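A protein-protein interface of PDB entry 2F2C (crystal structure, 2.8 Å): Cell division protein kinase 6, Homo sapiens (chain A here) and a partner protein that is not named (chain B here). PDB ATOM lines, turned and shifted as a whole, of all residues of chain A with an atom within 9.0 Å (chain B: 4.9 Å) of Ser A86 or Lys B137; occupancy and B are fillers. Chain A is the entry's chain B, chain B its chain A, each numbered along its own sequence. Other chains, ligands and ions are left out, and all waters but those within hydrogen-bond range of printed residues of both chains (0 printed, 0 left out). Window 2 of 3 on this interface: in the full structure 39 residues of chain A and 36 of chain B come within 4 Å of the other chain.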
ATOM      1  N   VAL A  47      31.026  11.291   6.512  1.00  0.00           N
ATOM      2  CA  VAL A  47      29.969  11.137   7.511  1.00  0.00           C
ATOM      3  C   VAL A  47      30.482  11.702   8.829  1.00  0.00           C
ATOM      4  O   VAL A  47      31.052  10.972   9.647  1.00  0.00           O
ATOM      5  CB  VAL A  47      29.586   9.638   7.697  1.00  0.00           C
ATOM      6  CG1 VAL A  47      28.564   9.455   8.811  1.00  0.00           C
ATOM      7  CG2 VAL A  47      29.068   9.036   6.396  1.00  0.00           C
ATOM      8  N   GLN A  48      30.288  13.004   9.028  1.00  0.00           N
ATOM      9  CA  GLN A  48      30.858  13.704  10.189  1.00  0.00           C
ATOM     10  C   GLN A  48      30.459  13.090  11.537  1.00  0.00           C
ATOM     11  O   GLN A  48      29.285  12.762  11.754  1.00  0.00           O
ATOM     12  CB  GLN A  48      30.511  15.196  10.154  1.00  0.00           C
ATOM     13  CG  GLN A  48      31.338  16.014   9.162  1.00  0.00           C
ATOM     14  CD  GLN A  48      31.251  17.512   9.415  1.00  0.00           C
ATOM     15  OE1 GLN A  48      30.155  18.083   9.437  1.00  0.00           O
ATOM     16  NE2 GLN A  48      32.403  18.151   9.605  1.00  0.00           N
ATOM     17  N   THR A  49      31.449  12.941  12.423  1.00  0.00           N
ATOM     18  CA  THR A  49      31.278  12.317  13.745  1.00  0.00           C
ATOM     19  C   THR A  49      30.256  13.075  14.604  1.00  0.00           C
ATOM     20  O   THR A  49      30.193  14.308  14.552  1.00  0.00           O
ATOM     21  CB  THR A  49      32.643  12.235  14.491  1.00  0.00           C
ATOM     22  OG1 THR A  49      33.695  11.929  13.569  1.00  0.00           O
ATOM     23  CG2 THR A  49      32.674  11.049  15.445  1.00  0.00           C
ATOM     24  N   GLY A  50      29.460  12.334  15.381  1.00  0.00           N
ATOM     25  CA  GLY A  50      28.435  12.913  16.266  1.00  0.00           C
ATOM     26  C   GLY A  50      27.529  13.943  15.602  1.00  0.00           C
ATOM     27  O   GLY A  50      27.633  15.140  15.872  1.00  0.00           O
ATOM     28  N   GLU A  52      23.922  13.171  12.951  1.00  0.00           N
ATOM     29  CA  GLU A  52      22.561  12.687  12.772  1.00  0.00           C
ATOM     30  C   GLU A  52      22.567  11.210  12.395  1.00  0.00           C
ATOM     31  O   GLU A  52      21.513  10.619  12.119  1.00  0.00           O
ATOM     32  CB  GLU A  52      21.876  13.487  11.663  1.00  0.00           C
ATOM     33  CG  GLU A  52      22.501  13.297  10.277  1.00  0.00           C
ATOM     34  CD  GLU A  52      21.702  13.964   9.165  1.00  0.00           C
ATOM     35  OE1 GLU A  52      20.909  14.892   9.485  1.00  0.00           O
ATOM     36  OE2 GLU A  52      21.869  13.565   7.976  1.00  0.00           O
ATOM     37  N   GLY A  53      23.761  10.624  12.381  1.00  0.00           N
ATOM     38  CA  GLY A  53      23.964   9.282  11.855  1.00  0.00           C
ATOM     39  C   GLY A  53      24.234   9.349  10.366  1.00  0.00           C
ATOM     40  O   GLY A  53      24.775  10.343   9.871  1.00  0.00           O
ATOM     41  N   MET A  54      23.846   8.295   9.650  1.00  0.00           N
ATOM     42  CA  MET A  54      24.086   8.190   8.209  1.00  0.00           C
ATOM     43  C   MET A  54      23.435   9.347   7.453  1.00  0.00           C
ATOM     44  O   MET A  54      22.329   9.765   7.805  1.00  0.00           O
ATOM     45  CB  MET A  54      23.578   6.847   7.687  1.00  0.00           C
ATOM     46  CG  MET A  54      24.314   5.625   8.251  1.00  0.00           C
ATOM     47  SD  MET A  54      25.993   5.375   7.606  1.00  0.00           S
ATOM     48  CE  MET A  54      26.993   5.971   8.972  1.00  0.00           C
ATOM     49  N   ILE A  59      21.111   7.377   2.275  1.00  0.00           N
ATOM     50  CA  ILE A  59      20.014   6.446   2.527  1.00  0.00           C
ATOM     51  C   ILE A  59      18.972   6.496   1.389  1.00  0.00           C
ATOM     52  O   ILE A  59      18.621   5.463   0.836  1.00  0.00           O
ATOM     53  CB  ILE A  59      19.393   6.685   3.923  1.00  0.00           C
ATOM     54  CG1 ILE A  59      20.491   6.719   4.991  1.00  0.00           C
ATOM     55  CG2 ILE A  59      18.403   5.598   4.266  1.00  0.00           C
ATOM     56  CD1 ILE A  59      20.029   6.472   6.381  1.00  0.00           C
ATOM     57  N   VAL A  82      27.720  -1.739  -0.214  1.00  0.00           N
ATOM     58  CA  VAL A  82      27.963  -0.603   0.675  1.00  0.00           C
ATOM     59  C   VAL A  82      28.920  -1.039   1.789  1.00  0.00           C
ATOM     60  O   VAL A  82      28.718  -2.084   2.398  1.00  0.00           O
ATOM     61  CB  VAL A  82      26.648  -0.029   1.244  1.00  0.00           C
ATOM     62  CG1 VAL A  82      26.927   1.157   2.146  1.00  0.00           C
ATOM     63  CG2 VAL A  82      25.718   0.396   0.118  1.00  0.00           C
ATOM     64  N   CYS A  83      29.954  -0.233   2.046  1.00  0.00           N
ATOM     65  CA  CYS A  83      31.064  -0.623   2.926  1.00  0.00           C
ATOM     66  C   CYS A  83      30.780  -0.525   4.434  1.00  0.00           C
ATOM     67  O   CYS A  83      30.873  -1.529   5.144  1.00  0.00           O
ATOM     68  CB  CYS A  83      32.329   0.145   2.560  1.00  0.00           C
ATOM     69  N   THR A  84      30.455   0.682   4.908  1.00  0.00           N
ATOM     70  CA  THR A  84      30.066   0.973   6.327  1.00  0.00           C
ATOM     71  C   THR A  84      31.209   1.067   7.363  1.00  0.00           C
ATOM     72  O   THR A  84      30.988   1.566   8.477  1.00  0.00           O
ATOM     73  CB  THR A  84      28.916   0.029   6.890  1.00  0.00           C
ATOM     74  OG1 THR A  84      29.415  -1.300   7.110  1.00  0.00           O
ATOM     75  CG2 THR A  84      27.759  -0.151   5.892  1.00  0.00           C
ATOM     76  N   VAL A  85      32.403   0.602   6.985  1.00  0.00           N
ATOM     77  CA  VAL A  85      33.553   0.399   7.899  1.00  0.00           C
ATOM     78  C   VAL A  85      33.770   1.478   8.985  1.00  0.00           C
ATOM     79  O   VAL A  85      33.805   2.677   8.686  1.00  0.00           O
ATOM     80  CB  VAL A  85      34.893   0.178   7.106  1.00  0.00           C
ATOM     81  CG1 VAL A  85      35.936  -0.539   7.973  1.00  0.00           C
ATOM     82  CG2 VAL A  85      34.653  -0.603   5.804  1.00  0.00           C
ATOM     83  N   SER A  86      33.915   1.030  10.237  1.00  0.00           N
ATOM     84  CA  SER A  86      34.227   1.905  11.381  1.00  0.00           C
ATOM     85  C   SER A  86      35.621   1.611  11.945  1.00  0.00           C
ATOM     86  O   SER A  86      36.187   2.411  12.696  1.00  0.00           O
ATOM     87  CB  SER A  86      33.179   1.753  12.490  1.00  0.00           C
ATOM     88  OG  SER A  86      31.971   2.414  12.153  1.00  0.00           O
ATOM     89  N   THR A  88      36.417   3.483  18.156  1.00  0.00           N
ATOM     90  CA  THR A  88      37.608   4.028  18.810  1.00  0.00           C
ATOM     91  C   THR A  88      37.982   5.419  18.278  1.00  0.00           C
ATOM     92  O   THR A  88      37.384   6.426  18.687  1.00  0.00           O
ATOM     93  CB  THR A  88      38.793   3.058  18.707  1.00  0.00           C
ATOM     94  N   ASP A  89      38.953   5.470  17.362  1.00  0.00           N
ATOM     95  CA  ASP A  89      39.465   6.749  16.855  1.00  0.00           C
ATOM     96  C   ASP A  89      38.861   7.176  15.513  1.00  0.00           C
ATOM     97  O   ASP A  89      38.670   8.368  15.266  1.00  0.00           O
ATOM     98  CB  ASP A  89      41.004   6.741  16.789  1.00  0.00           C
ATOM     99  CG  ASP A  89      41.549   5.877  15.654  1.00  0.00           C
ATOM    100  OD1 ASP A  89      40.936   4.836  15.320  1.00  0.00           O
ATOM    101  OD2 ASP A  89      42.599   6.162  15.042  1.00  0.00           O
ATOM    102  N   ARG A  90      38.568   6.199  14.656  1.00  0.00           N
ATOM    103  CA  ARG A  90      38.080   6.467  13.307  1.00  0.00           C
ATOM    104  C   ARG A  90      36.616   6.885  13.306  1.00  0.00           C
ATOM    105  O   ARG A  90      35.897   6.677  14.290  1.00  0.00           O
ATOM    106  CB  ARG A  90      38.285   5.245  12.418  1.00  0.00           C
ATOM    107  N   GLU A  91      36.197   7.493  12.195  1.00  0.00           N
ATOM    108  CA  GLU A  91      34.794   7.812  11.937  1.00  0.00           C
ATOM    109  C   GLU A  91      34.166   6.659  11.158  1.00  0.00           C
ATOM    110  O   GLU A  91      34.719   5.559  11.120  1.00  0.00           O
ATOM    111  CB  GLU A  91      34.690   9.111  11.149  1.00  0.00           C
ATOM    112  N   THR A  92      33.006   6.899  10.553  1.00  0.00           N
ATOM    113  CA  THR A  92      32.440   5.942   9.614  1.00  0.00           C
ATOM    114  C   THR A  92      33.133   6.149   8.270  1.00  0.00           C
ATOM    115  O   THR A  92      33.492   7.275   7.927  1.00  0.00           O
ATOM    116  CB  THR A  92      30.942   6.127   9.492  1.00  0.00           C
ATOM    117  N   LYS A  93      33.348   5.066   7.528  1.00  0.00           N
ATOM    118  CA  LYS A  93      33.903   5.140   6.179  1.00  0.00           C
ATOM    119  C   LYS A  93      32.908   4.508   5.203  1.00  0.00           C
ATOM    120  O   LYS A  93      32.757   3.281   5.160  1.00  0.00           O
ATOM    121  CB  LYS A  93      35.264   4.452   6.117  1.00  0.00           C
ATOM    122  N   LEU A  94      32.213   5.354   4.443  1.00  0.00           N
ATOM    123  CA  LEU A  94      31.183   4.882   3.513  1.00  0.00           C
ATOM    124  C   LEU A  94      31.653   4.787   2.067  1.00  0.00           C
ATOM    125  O   LEU A  94      31.722   5.795   1.358  1.00  0.00           O
ATOM    126  CB  LEU A  94      29.912   5.741   3.590  1.00  0.00           C
ATOM    127  CG  LEU A  94      28.761   5.328   4.518  1.00  0.00           C
ATOM    128  CD1 LEU A  94      27.568   6.217   4.246  1.00  0.00           C
ATOM    129  CD2 LEU A  94      28.364   3.859   4.366  1.00  0.00           C
ATOM    130  N   ILE B 133      23.050   5.985  17.114  1.00  0.00           N
ATOM    131  CA  ILE B 133      23.770   5.967  15.837  1.00  0.00           C
ATOM    132  C   ILE B 133      24.268   4.565  15.480  1.00  0.00           C
ATOM    133  O   ILE B 133      24.088   4.115  14.352  1.00  0.00           O
ATOM    134  CB  ILE B 133      24.920   7.000  15.861  1.00  0.00           C
ATOM    135  CG1 ILE B 133      24.334   8.416  15.914  1.00  0.00           C
ATOM    136  CG2 ILE B 133      25.837   6.842  14.651  1.00  0.00           C
ATOM    137  CD1 ILE B 133      25.225   9.439  16.636  1.00  0.00           C
ATOM    138  N   ASN B 134      24.868   3.868  16.440  1.00  0.00           N
ATOM    139  CA  ASN B 134      25.286   2.492  16.211  1.00  0.00           C
ATOM    140  C   ASN B 134      24.118   1.566  15.870  1.00  0.00           C
ATOM    141  O   ASN B 134      24.262   0.636  15.079  1.00  0.00           O
ATOM    142  CB  ASN B 134      26.107   1.962  17.389  1.00  0.00           C
ATOM    143  CG  ASN B 134      27.555   2.417  17.330  1.00  0.00           C
ATOM    144  OD1 ASN B 134      27.998   3.227  18.145  1.00  0.00           O
ATOM    145  ND2 ASN B 134      28.297   1.909  16.350  1.00  0.00           N
ATOM    146  N   GLN B 135      22.955   1.847  16.450  1.00  0.00           N
ATOM    147  CA  GLN B 135      21.745   1.068  16.193  1.00  0.00           C
ATOM    148  C   GLN B 135      21.183   1.349  14.801  1.00  0.00           C
ATOM    149  O   GLN B 135      20.625   0.447  14.164  1.00  0.00           O
ATOM    150  CB  GLN B 135      20.685   1.331  17.272  1.00  0.00           C
ATOM    151  CG  GLN B 135      19.441   0.459  17.179  1.00  0.00           C
ATOM    152  CD  GLN B 135      19.774  -1.009  17.218  1.00  0.00           C
ATOM    153  OE1 GLN B 135      19.995  -1.571  18.294  1.00  0.00           O
ATOM    154  NE2 GLN B 135      19.815  -1.639  16.046  1.00  0.00           N
ATOM    155  N   GLU B 136      21.327   2.592  14.332  1.00  0.00           N
ATOM    156  CA  GLU B 136      20.987   2.939  12.945  1.00  0.00           C
ATOM    157  C   GLU B 136      21.928   2.214  11.989  1.00  0.00           C
ATOM    158  O   GLU B 136      21.508   1.726  10.940  1.00  0.00           O
ATOM    159  CB  GLU B 136      21.068   4.448  12.702  1.00  0.00           C
ATOM    160  CG  GLU B 136      20.443   4.884  11.384  1.00  0.00           C
ATOM    161  CD  GLU B 136      21.022   6.181  10.847  1.00  0.00           C
ATOM    162  OE1 GLU B 136      22.269   6.298  10.786  1.00  0.00           O
ATOM    163  OE2 GLU B 136      20.235   7.074  10.459  1.00  0.00           O
ATOM    164  N   LYS B 137      23.197   2.147  12.374  1.00  0.00           N
ATOM    165  CA  LYS B 137      24.241   1.518  11.574  1.00  0.00           C
ATOM    166  C   LYS B 137      24.085  -0.002  11.534  1.00  0.00           C
ATOM    167  O   LYS B 137      24.346  -0.620  10.508  1.00  0.00           O
ATOM    168  CB  LYS B 137      25.596   1.900  12.147  1.00  0.00           C
ATOM    169  CG  LYS B 137      26.775   1.547  11.280  1.00  0.00           C
ATOM    170  CD  LYS B 137      27.891   2.601  11.404  1.00  0.00           C
ATOM    171  CE  LYS B 137      28.388   2.794  12.842  1.00  0.00           C
ATOM    172  NZ  LYS B 137      29.014   4.139  13.022  1.00  0.00           N
ATOM    173  N   ASP B 138      23.647  -0.593  12.648  1.00  0.00           N
ATOM    174  CA  ASP B 138      23.431  -2.036  12.717  1.00  0.00           C
ATOM    175  C   ASP B 138      22.179  -2.487  11.963  1.00  0.00           C
ATOM    176  O   ASP B 138      22.218  -3.500  11.250  1.00  0.00           O
ATOM    177  CB  ASP B 138      23.433  -2.530  14.165  1.00  0.00           C
ATOM    178  CG  ASP B 138      24.851  -2.776  14.704  1.00  0.00           C
ATOM    179  OD1 ASP B 138      25.063  -2.640  15.933  1.00  0.00           O
ATOM    180  OD2 ASP B 138      25.820  -3.108  13.981  1.00  0.00           O
ATOM    181  N   ILE B 139      21.082  -1.736  12.107  1.00  0.00           N
ATOM    182  CA  ILE B 139      19.869  -1.977  11.300  1.00  0.00           C
ATOM    183  C   ILE B 139      20.152  -1.915   9.792  1.00  0.00           C
ATOM    184  O   ILE B 139      19.871  -2.863   9.049  1.00  0.00           O
ATOM    185  CB  ILE B 139      18.745  -0.987  11.645  1.00  0.00           C
ATOM    186  CG1 ILE B 139      18.168  -1.283  13.028  1.00  0.00           C
ATOM    187  CG2 ILE B 139      17.641  -1.044  10.580  1.00  0.00           C
ATOM    188  CD1 ILE B 139      17.311  -0.172  13.555  1.00  0.00           C
ATOM    189  N   LEU B 140      20.712  -0.799   9.343  1.00  0.00           N
ATOM    190  CA  LEU B 140      20.982  -0.617   7.936  1.00  0.00           C
ATOM    191  C   LEU B 140      21.781  -1.774   7.339  1.00  0.00           C
ATOM    192  O   LEU B 140      21.403  -2.335   6.311  1.00  0.00           O
ATOM    193  CB  LEU B 140      21.700   0.707   7.706  1.00  0.00           C
ATOM    194  CG  LEU B 140      20.817   1.958   7.726  1.00  0.00           C
ATOM    195  CD1 LEU B 140      21.695   3.199   7.831  1.00  0.00           C
ATOM    196  CD2 LEU B 140      19.908   2.035   6.502  1.00  0.00           C
ATOM    197  N   GLU B 141      22.875  -2.153   7.986  1.00  0.00           N
ATOM    198  CA  GLU B 141      23.745  -3.144   7.386  1.00  0.00           C
ATOM    199  C   GLU B 141      23.218  -4.573   7.441  1.00  0.00           C
ATOM    200  O   GLU B 141      23.566  -5.394   6.606  1.00  0.00           O
ATOM    201  CB  GLU B 141      25.212  -2.976   7.827  1.00  0.00           C
ATOM    202  CG  GLU B 141      25.699  -3.664   9.097  1.00  0.00           C
ATOM    203  CD  GLU B 141      27.230  -3.565   9.234  1.00  0.00           C
ATOM    204  OE1 GLU B 141      27.739  -2.488   9.638  1.00  0.00           O
ATOM    205  OE2 GLU B 141      27.941  -4.557   8.926  1.00  0.00           O
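Printed residues of chain B that touch a printed residue of chain A: Glu B136, Lys B137, Leu B140 and Glu B141.
Along chain B the printed residues that touch a printed residue of chain A span positions 136 to 141.
Among the printed residues, 6 pairs touch across the chains.
Among the printed residues, no Asp or Glu carboxylate lies within 4 Å of a Lys or Arg side-chain nitrogen of the other chain.
Among the printed residues, merely in contact across the chains: Gly A53 with Glu B136 (3.6 Å), Met A54 with Leu B140 (3.6 Å), Ile A59 with Leu B140 (3.9 Å) and Ser A86 with Lys B137 (3.5 Å).
N of Thr A84 lies within hydrogen-bond range of O of Lys A93, at 3.5 Å.
Of chain B, only Lys B137 comes within 4 Å of Ser A86.
Of the printed residues of chain A, Lys B137 touches Ser A86.
Of the printed residues of chain B, Ile A59 touches Leu B140.
Of the printed residues of chain A, Leu B140 touches Met A54 (3.6 Å) and Ile A59 (3.9 Å).
Printed residues of chain A within 4 Å of Glu B136: Gly A53 and Met A54.
Of the printed residues of chain A, Glu B141 touches Thr A84 (3.3 Å).
Lys A93 touches none of the printed residues of chain B.
Thr A92 touches none of the printed residues of chain B.
The nearest residue of chain A that does not touch Lys B137 is Met A54 (4.3 Å).
OE1 of Glu B136 is in hydrogen-bond range of N of Met A54 (2.8 Å).
OG1 of Thr A84 sits at hydrogen-bond distance from OE1 of Glu B141, at 3.3 Å.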
